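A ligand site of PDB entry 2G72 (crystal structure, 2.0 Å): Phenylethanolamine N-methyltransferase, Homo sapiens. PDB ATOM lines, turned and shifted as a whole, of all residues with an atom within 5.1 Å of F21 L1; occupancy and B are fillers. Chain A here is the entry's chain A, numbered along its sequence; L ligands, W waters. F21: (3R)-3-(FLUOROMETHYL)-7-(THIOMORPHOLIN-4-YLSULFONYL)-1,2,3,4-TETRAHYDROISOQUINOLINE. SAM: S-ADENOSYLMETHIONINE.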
ATOM      1  N   TYR A  35      -3.280 -20.205   8.955  1.00  0.00           N
ATOM      2  CA  TYR A  35      -4.399 -19.394   9.435  1.00  0.00           C
ATOM      3  C   TYR A  35      -3.919 -18.360  10.459  1.00  0.00           C
ATOM      4  O   TYR A  35      -4.271 -17.170  10.390  1.00  0.00           O
ATOM      5  CB  TYR A  35      -5.474 -20.291  10.067  1.00  0.00           C
ATOM      6  CG  TYR A  35      -6.626 -19.518  10.686  1.00  0.00           C
ATOM      7  CD1 TYR A  35      -7.603 -18.918   9.884  1.00  0.00           C
ATOM      8  CD2 TYR A  35      -6.739 -19.377  12.068  1.00  0.00           C
ATOM      9  CE1 TYR A  35      -8.650 -18.205  10.448  1.00  0.00           C
ATOM     10  CE2 TYR A  35      -7.800 -18.662  12.650  1.00  0.00           C
ATOM     11  CZ  TYR A  35      -8.742 -18.086  11.821  1.00  0.00           C
ATOM     12  OH  TYR A  35      -9.769 -17.362  12.366  1.00  0.00           O
ATOM     13  N   ASN A  39      -3.854 -14.152   9.885  1.00  0.00           N
ATOM     14  CA  ASN A  39      -4.689 -13.291  10.718  1.00  0.00           C
ATOM     15  C   ASN A  39      -4.149 -12.767  12.041  1.00  0.00           C
ATOM     16  O   ASN A  39      -4.426 -11.615  12.410  1.00  0.00           O
ATOM     17  CB  ASN A  39      -6.019 -13.996  10.952  1.00  0.00           C
ATOM     18  CG  ASN A  39      -6.698 -14.362   9.644  1.00  0.00           C
ATOM     19  OD1 ASN A  39      -7.204 -13.486   8.922  1.00  0.00           O
ATOM     20  ND2 ASN A  39      -6.690 -15.648   9.309  1.00  0.00           N
ATOM     21  N   TYR A  40      -3.381 -13.566  12.771  1.00  0.00           N
ATOM     22  CA  TYR A  40      -2.913 -13.110  14.063  1.00  0.00           C
ATOM     23  C   TYR A  40      -1.506 -12.583  14.154  1.00  0.00           C
ATOM     24  O   TYR A  40      -1.086 -12.137  15.210  1.00  0.00           O
ATOM     25  CB  TYR A  40      -3.236 -14.176  15.112  1.00  0.00           C
ATOM     26  CG  TYR A  40      -4.729 -14.377  15.179  1.00  0.00           C
ATOM     27  CD1 TYR A  40      -5.358 -15.321  14.363  1.00  0.00           C
ATOM     28  CD2 TYR A  40      -5.529 -13.559  15.963  1.00  0.00           C
ATOM     29  CE1 TYR A  40      -6.740 -15.445  14.320  1.00  0.00           C
ATOM     30  CE2 TYR A  40      -6.896 -13.664  15.941  1.00  0.00           C
ATOM     31  CZ  TYR A  40      -7.512 -14.601  15.118  1.00  0.00           C
ATOM     32  OH  TYR A  40      -8.886 -14.695  15.077  1.00  0.00           O
ATOM     33  N   ARG A  44      -2.508  -7.476  10.720  1.00  0.00           N
ATOM     34  CA  ARG A  44      -3.712  -7.580  11.541  1.00  0.00           C
ATOM     35  C   ARG A  44      -3.402  -7.827  13.006  1.00  0.00           C
ATOM     36  O   ARG A  44      -4.133  -7.383  13.895  1.00  0.00           O
ATOM     37  CB  ARG A  44      -4.613  -8.685  11.000  1.00  0.00           C
ATOM     38  CG  ARG A  44      -5.181  -8.330   9.645  1.00  0.00           C
ATOM     39  CD  ARG A  44      -6.033  -9.429   9.050  1.00  0.00           C
ATOM     40  NE  ARG A  44      -6.640  -8.980   7.802  1.00  0.00           N
ATOM     41  CZ  ARG A  44      -7.519  -9.687   7.106  1.00  0.00           C
ATOM     42  NH1 ARG A  44      -7.894 -10.889   7.550  1.00  0.00           N
ATOM     43  NH2 ARG A  44      -8.024  -9.184   5.978  1.00  0.00           N
ATOM     44  N   GLY A  45      -2.306  -8.549  13.261  1.00  0.00           N
ATOM     45  CA  GLY A  45      -1.906  -8.828  14.629  1.00  0.00           C
ATOM     46  C   GLY A  45      -1.046  -7.767  15.286  1.00  0.00           C
ATOM     47  O   GLY A  45      -0.554  -8.002  16.386  1.00  0.00           O
ATOM     48  N   VAL A  53      -7.529  -3.622  14.225  1.00  0.00           N
ATOM     49  CA  VAL A  53      -8.616  -4.499  14.623  1.00  0.00           C
ATOM     50  C   VAL A  53      -8.261  -5.339  15.857  1.00  0.00           C
ATOM     51  O   VAL A  53      -9.150  -5.707  16.646  1.00  0.00           O
ATOM     52  CB  VAL A  53      -9.022  -5.425  13.434  1.00  0.00           C
ATOM     53  CG1 VAL A  53      -7.865  -6.393  13.063  1.00  0.00           C
ATOM     54  CG2 VAL A  53     -10.308  -6.194  13.761  1.00  0.00           C
ATOM     55  N   GLY A  54      -6.971  -5.598  16.043  1.00  0.00           N
ATOM     56  CA  GLY A  54      -6.532  -6.380  17.205  1.00  0.00           C
ATOM     57  C   GLY A  54      -6.854  -5.603  18.464  1.00  0.00           C
ATOM     58  O   GLY A  54      -7.565  -6.098  19.333  1.00  0.00           O
ATOM     59  N   LYS A  57     -10.723  -5.331  18.964  1.00  0.00           N
ATOM     60  CA  LYS A  57     -11.401  -6.533  19.427  1.00  0.00           C
ATOM     61  C   LYS A  57     -11.112  -6.824  20.904  1.00  0.00           C
ATOM     62  O   LYS A  57     -12.043  -7.120  21.670  1.00  0.00           O
ATOM     63  CB  LYS A  57     -10.979  -7.744  18.597  1.00  0.00           C
ATOM     64  CG  LYS A  57     -11.711  -9.036  18.944  1.00  0.00           C
ATOM     65  CD  LYS A  57     -13.087  -9.177  18.263  1.00  0.00           C
ATOM     66  CE  LYS A  57     -14.105  -8.166  18.770  1.00  0.00           C
ATOM     67  NZ  LYS A  57     -14.345  -8.277  20.247  1.00  0.00           N
ATOM     68  N   TYR A  85      -7.018 -15.897  22.063  1.00  0.00           N
ATOM     69  CA  TYR A  85      -7.210 -14.471  22.394  1.00  0.00           C
ATOM     70  C   TYR A  85      -8.647 -14.176  22.794  1.00  0.00           C
ATOM     71  O   TYR A  85      -8.880 -13.304  23.645  1.00  0.00           O
ATOM     72  CB  TYR A  85      -6.835 -13.584  21.218  1.00  0.00           C
ATOM     73  CG  TYR A  85      -7.894 -13.572  20.146  1.00  0.00           C
ATOM     74  CD1 TYR A  85      -8.953 -12.654  20.188  1.00  0.00           C
ATOM     75  CD2 TYR A  85      -7.913 -14.561  19.151  1.00  0.00           C
ATOM     76  CE1 TYR A  85     -10.003 -12.729  19.259  1.00  0.00           C
ATOM     77  CE2 TYR A  85      -8.956 -14.656  18.230  1.00  0.00           C
ATOM     78  CZ  TYR A  85     -10.007 -13.731  18.294  1.00  0.00           C
ATOM     79  OH  TYR A  85     -11.048 -13.869  17.430  1.00  0.00           O
ATOM     80  N   TYR A 126      -0.699 -10.618  22.830  1.00  0.00           N
ATOM     81  CA  TYR A 126      -2.142 -10.471  23.078  1.00  0.00           C
ATOM     82  C   TYR A 126      -2.423 -10.490  24.569  1.00  0.00           C
ATOM     83  O   TYR A 126      -3.231  -9.695  25.072  1.00  0.00           O
ATOM     84  CB  TYR A 126      -2.954 -11.590  22.385  1.00  0.00           C
ATOM     85  CG  TYR A 126      -2.956 -11.507  20.866  1.00  0.00           C
ATOM     86  CD1 TYR A 126      -1.846 -11.899  20.119  1.00  0.00           C
ATOM     87  CD2 TYR A 126      -4.072 -11.009  20.177  1.00  0.00           C
ATOM     88  CE1 TYR A 126      -1.831 -11.786  18.723  1.00  0.00           C
ATOM     89  CE2 TYR A 126      -4.070 -10.903  18.789  1.00  0.00           C
ATOM     90  CZ  TYR A 126      -2.946 -11.285  18.070  1.00  0.00           C
ATOM     91  OH  TYR A 126      -2.951 -11.189  16.700  1.00  0.00           O
ATOM     92  N   PHE A 182     -15.771 -15.965  14.576  1.00  0.00           N
ATOM     93  CA  PHE A 182     -15.519 -16.401  13.205  1.00  0.00           C
ATOM     94  C   PHE A 182     -15.809 -17.872  12.892  1.00  0.00           C
ATOM     95  O   PHE A 182     -15.142 -18.478  12.047  1.00  0.00           O
ATOM     96  CB  PHE A 182     -14.076 -16.095  12.820  1.00  0.00           C
ATOM     97  CG  PHE A 182     -13.684 -14.668  13.008  1.00  0.00           C
ATOM     98  CD1 PHE A 182     -12.855 -14.298  14.061  1.00  0.00           C
ATOM     99  CD2 PHE A 182     -14.136 -13.687  12.116  1.00  0.00           C
ATOM    100  CE1 PHE A 182     -12.457 -12.951  14.234  1.00  0.00           C
ATOM    101  CE2 PHE A 182     -13.738 -12.333  12.282  1.00  0.00           C
ATOM    102  CZ  PHE A 182     -12.902 -11.966  13.347  1.00  0.00           C
ATOM    103  N   ALA A 186     -18.343 -18.843   8.893  1.00  0.00           N
ATOM    104  CA  ALA A 186     -17.242 -19.474   8.178  1.00  0.00           C
ATOM    105  C   ALA A 186     -17.446 -20.953   7.870  1.00  0.00           C
ATOM    106  O   ALA A 186     -16.634 -21.575   7.185  1.00  0.00           O
ATOM    107  CB  ALA A 186     -15.934 -19.299   8.944  1.00  0.00           C
ATOM    108  N   ALA A 216     -16.970 -12.250  10.840  1.00  0.00           N
ATOM    109  CA  ALA A 216     -16.661 -11.485   9.632  1.00  0.00           C
ATOM    110  C   ALA A 216     -17.910 -10.899   8.955  1.00  0.00           C
ATOM    111  O   ALA A 216     -18.924 -11.574   8.811  1.00  0.00           O
ATOM    112  CB  ALA A 216     -15.922 -12.389   8.661  1.00  0.00           C
ATOM    113  N   GLU A 219     -18.061 -11.253   4.170  1.00  0.00           N
ATOM    114  CA  GLU A 219     -16.898 -12.006   3.694  1.00  0.00           C
ATOM    115  C   GLU A 219     -17.409 -13.207   2.903  1.00  0.00           C
ATOM    116  O   GLU A 219     -18.452 -13.769   3.265  1.00  0.00           O
ATOM    117  CB  GLU A 219     -16.066 -12.488   4.887  1.00  0.00           C
ATOM    118  CG  GLU A 219     -14.881 -13.351   4.498  1.00  0.00           C
ATOM    119  CD  GLU A 219     -14.126 -13.840   5.729  1.00  0.00           C
ATOM    120  OE1 GLU A 219     -12.905 -13.598   5.834  1.00  0.00           O
ATOM    121  OE2 GLU A 219     -14.775 -14.472   6.594  1.00  0.00           O
ATOM    122  N   TYR A 222     -11.763 -17.116   2.374  1.00  0.00           N
ATOM    123  CA  TYR A 222     -10.526 -16.848   3.079  1.00  0.00           C
ATOM    124  C   TYR A 222      -9.658 -18.071   2.878  1.00  0.00           C
ATOM    125  O   TYR A 222     -10.169 -19.157   2.609  1.00  0.00           O
ATOM    126  CB  TYR A 222     -10.770 -16.591   4.580  1.00  0.00           C
ATOM    127  CG  TYR A 222     -11.050 -17.816   5.419  1.00  0.00           C
ATOM    128  CD1 TYR A 222     -10.019 -18.434   6.122  1.00  0.00           C
ATOM    129  CD2 TYR A 222     -12.352 -18.310   5.559  1.00  0.00           C
ATOM    130  CE1 TYR A 222     -10.270 -19.520   6.951  1.00  0.00           C
ATOM    131  CE2 TYR A 222     -12.617 -19.403   6.395  1.00  0.00           C
ATOM    132  CZ  TYR A 222     -11.565 -19.993   7.101  1.00  0.00           C
ATOM    133  OH  TYR A 222     -11.801 -21.045   7.937  1.00  0.00           O
ATOM    134  N   VAL A 231     -17.377 -18.633   2.720  1.00  0.00           N
ATOM    135  CA  VAL A 231     -17.936 -18.006   3.904  1.00  0.00           C
ATOM    136  C   VAL A 231     -19.258 -17.416   3.443  1.00  0.00           C
ATOM    137  O   VAL A 231     -19.390 -17.064   2.275  1.00  0.00           O
ATOM    138  CB  VAL A 231     -17.036 -16.845   4.432  1.00  0.00           C
ATOM    139  CG1 VAL A 231     -17.671 -16.192   5.661  1.00  0.00           C
ATOM    140  CG2 VAL A 231     -15.631 -17.351   4.760  1.00  0.00           C
ATOM    141  N   MET A 258     -12.916  -2.870   8.112  1.00  0.00           N
ATOM    142  CA  MET A 258     -11.533  -3.202   7.822  1.00  0.00           C
ATOM    143  C   MET A 258     -10.858  -2.119   6.982  1.00  0.00           C
ATOM    144  O   MET A 258     -11.238  -1.872   5.849  1.00  0.00           O
ATOM    145  CB  MET A 258     -11.449  -4.544   7.119  1.00  0.00           C
ATOM    146  CG  MET A 258     -10.126  -5.284   7.381  1.00  0.00           C
ATOM    147  SD  MET A 258      -9.837  -5.603   9.158  1.00  0.00           S
ATOM    148  CE  MET A 258     -10.336  -7.295   9.322  1.00  0.00           C
ATOM    149  N   ASP A 267      -8.157 -12.949   2.258  1.00  0.00           N
ATOM    150  CA  ASP A 267      -9.601 -13.046   2.260  1.00  0.00           C
ATOM    151  C   ASP A 267     -10.191 -11.780   1.677  1.00  0.00           C
ATOM    152  O   ASP A 267      -9.461 -10.939   1.153  1.00  0.00           O
ATOM    153  CB  ASP A 267     -10.147 -13.263   3.698  1.00  0.00           C
ATOM    154  CG  ASP A 267      -9.816 -12.109   4.649  1.00  0.00           C
ATOM    155  OD1 ASP A 267      -9.816 -10.929   4.246  1.00  0.00           O
ATOM    156  OD2 ASP A 267      -9.570 -12.402   5.837  1.00  0.00           O
ATOM    157  N   VAL A 269     -12.746 -10.006   3.552  1.00  0.00           N
ATOM    158  CA  VAL A 269     -13.584  -9.483   4.638  1.00  0.00           C
ATOM    159  C   VAL A 269     -13.680  -7.962   4.531  1.00  0.00           C
ATOM    160  O   VAL A 269     -12.699  -7.284   4.210  1.00  0.00           O
ATOM    161  CB  VAL A 269     -13.009  -9.912   6.030  1.00  0.00           C
ATOM    162  CG1 VAL A 269     -11.619  -9.294   6.239  1.00  0.00           C
ATOM    163  CG2 VAL A 269     -13.946  -9.491   7.152  1.00  0.00           C
ATOM    164  N   VAL A 272     -15.690  -6.402  10.756  1.00  0.00           N
ATOM    165  CA  VAL A 272     -15.807  -7.399  11.804  1.00  0.00           C
ATOM    166  C   VAL A 272     -16.918  -6.947  12.754  1.00  0.00           C
ATOM    167  O   VAL A 272     -16.991  -5.770  13.103  1.00  0.00           O
ATOM    168  CB  VAL A 272     -14.479  -7.528  12.604  1.00  0.00           C
ATOM    169  CG1 VAL A 272     -14.689  -8.395  13.860  1.00  0.00           C
ATOM    170  CG2 VAL A 272     -13.389  -8.125  11.717  1.00  0.00           C
HETATM  171  C12 F21 L   1      -9.359 -10.261  14.962  1.00  0.00           C
HETATM  172  C13 F21 L   1      -8.889  -9.607  16.267  1.00  0.00           C
HETATM  173  S2  F21 L   1      -7.160 -10.111  16.562  1.00  0.00           S
HETATM  174  C15 F21 L   1      -6.314  -9.844  14.965  1.00  0.00           C
HETATM  175  C14 F21 L   1      -7.181 -10.462  13.859  1.00  0.00           C
HETATM  176  N1  F21 L   1      -8.491  -9.787  13.871  1.00  0.00           N
HETATM  177  S1  F21 L   1      -9.214  -9.881  12.418  1.00  0.00           S
HETATM  178  O2  F21 L   1     -10.344  -9.012  12.451  1.00  0.00           O
HETATM  179  O1  F21 L   1      -8.245  -9.368  11.384  1.00  0.00           O
HETATM  180  C7  F21 L   1      -9.737 -11.451  11.860  1.00  0.00           C
HETATM  181  C8  F21 L   1     -10.300 -11.542  10.589  1.00  0.00           C
HETATM  182  C9  F21 L   1     -10.712 -12.767  10.072  1.00  0.00           C
HETATM  183  C1  F21 L   1     -11.447 -12.808   8.725  1.00  0.00           C
HETATM  184  N2  F21 L   1     -11.613 -14.179   8.206  1.00  0.00           N
HETATM  185  C3  F21 L   1     -12.020 -15.129   9.250  1.00  0.00           C
HETATM  186  C11 F21 L   1     -12.323 -16.510   8.661  1.00  0.00           C
HETATM  187  F1  F21 L   1     -13.629 -16.540   8.209  1.00  0.00           F
HETATM  188  C4  F21 L   1     -10.906 -15.293  10.285  1.00  0.00           C
HETATM  189  C10 F21 L   1     -10.534 -13.916  10.839  1.00  0.00           C
HETATM  190  C5  F21 L   1      -9.971 -13.832  12.117  1.00  0.00           C
HETATM  191  C6  F21 L   1      -9.572 -12.607  12.634  1.00  0.00           C
HETATM  192  N   SAM L   2     -12.484 -18.874  16.658  1.00  0.00           N
HETATM  193  CA  SAM L   2     -11.199 -18.816  15.979  1.00  0.00           C
HETATM  194  C   SAM L   2     -10.804 -17.368  15.694  1.00  0.00           C
HETATM  195  O   SAM L   2     -11.359 -16.476  16.377  1.00  0.00           O
HETATM  196  OXT SAM L   2      -9.925 -17.126  14.837  1.00  0.00           O
HETATM  197  CB  SAM L   2     -11.224 -19.672  14.697  1.00  0.00           C
HETATM  198  CG  SAM L   2     -12.238 -19.284  13.612  1.00  0.00           C
HETATM  199  SD  SAM L   2     -11.974 -20.231  12.041  1.00  0.00           S
HETATM  200  CE  SAM L   2     -11.964 -19.099  10.650  1.00  0.00           C
HETATM  201  C5' SAM L   2     -13.363 -21.433  11.791  1.00  0.00           C
HETATM  202  C4' SAM L   2     -13.294 -22.620  12.727  1.00  0.00           C
HETATM  203  O4' SAM L   2     -14.491 -23.449  12.669  1.00  0.00           O
HETATM  204  C3' SAM L   2     -12.108 -23.528  12.378  1.00  0.00           C
HETATM  205  O3' SAM L   2     -11.325 -23.780  13.530  1.00  0.00           O
HETATM  206  C2' SAM L   2     -12.784 -24.776  11.824  1.00  0.00           C
HETATM  207  O2' SAM L   2     -12.039 -25.950  12.027  1.00  0.00           O
HETATM  208  C1' SAM L   2     -14.094 -24.805  12.611  1.00  0.00           C
HETATM  209  N9  SAM L   2     -15.178 -25.589  11.998  1.00  0.00           N
HETATM  210  C8  SAM L   2     -15.257 -26.135  10.689  1.00  0.00           C
HETATM  211  N7  SAM L   2     -16.365 -26.804  10.478  1.00  0.00           N
HETATM  212  C5  SAM L   2     -17.042 -26.701  11.675  1.00  0.00           C
HETATM  213  C6  SAM L   2     -18.304 -27.241  12.034  1.00  0.00           C
HETATM  214  N6  SAM L   2     -19.059 -27.963  11.215  1.00  0.00           N
HETATM  215  N1  SAM L   2     -18.751 -26.992  13.303  1.00  0.00           N
HETATM  216  C2  SAM L   2     -17.960 -26.256  14.137  1.00  0.00           C
HETATM  217  N3  SAM L   2     -16.744 -25.700  13.887  1.00  0.00           N
HETATM  218  C4  SAM L   2     -16.347 -25.960  12.622  1.00  0.00           C
HETATM  219  O   HOH W   1      -9.155 -14.565   7.069  1.00  0.00           O
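An oxygen (OXT) of SAM L2 is in hydrogen-bond range of the side-chain hydroxyl of Tyr 35, 2.5 Å away. O of SAM L2 is in hydrogen-bond range of OH of Tyr 85, 2.8 Å away. OE1 of Glu 219 lies within salt-bridge range of N2 of F21 L1 (2.8 Å). OXT of SAM L2 is in hydrogen-bond range of OH of Tyr 40, at 2.7 Å. The side-chain carboxylate of Asp 267 lies within salt-bridge range of a nitrogen (N2) of F21 L1, at 3.6 Å.
The side-chain hydroxyl (OH) of Tyr 40 sits close to the side-chain hydroxyl (OH) of Tyr 85. The backbone carbonyl oxygen (O) of Tyr 40 lies within hydrogen-bond range of the side-chain hydroxyl (OH) of Tyr 126. The backbone carbonyl oxygen (O) of Tyr 35 is in hydrogen-bond range of the side-chain amide nitrogen (ND2) of Asn 39 (3.1 Å). The guanidinium group of Arg 44 is in salt-bridge range of the side-chain carboxylate of Asp 267 (2.8 Å). The backbone NH of Val 269 sits close to the side-chain carboxylate of Asp 267 (3.1 Å). NH1 of Arg 44 lies within hydrogen-bond range of OD1 of Asn 39, at 3.0 Å.
Tyr 35 touches F21 L1 (OH to C4, 3.1 Å). Asn 39 touches F21 L1. Tyr 40 touches F21 L1 (OH to C5, 3.3 Å). Arg 44 touches F21 L1. Val 53 touches F21 L1 (CG2 to O2, 3.1 Å). Gly 54 touches F21 L1. Lys 57 touches F21 L1. Tyr 126 touches F21 L1 (CE2 to S2, 3.9 Å). Phe 182 touches F21 L1 (CE1 to C6, 3.3 Å). Ala 186 touches F21 L1 (CB to F1, 3.7 Å). Tyr 222 touches F21 L1. Met 258 touches F21 L1 (CE to O2, 3.6 Å). Val 272 touches F21 L1. Hydrophobic or aromatic side chains within 4 Å of F21 L1: Tyr 35, Tyr 40, Val 53, Tyr 126, Phe 182, Ala 186, Tyr 222, Met 258 and Val 272.
Water W1 lies within hydrogen-bond range of OD2 of Asp 267, N2 of F21 L1 and OD1 of Asn 39.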
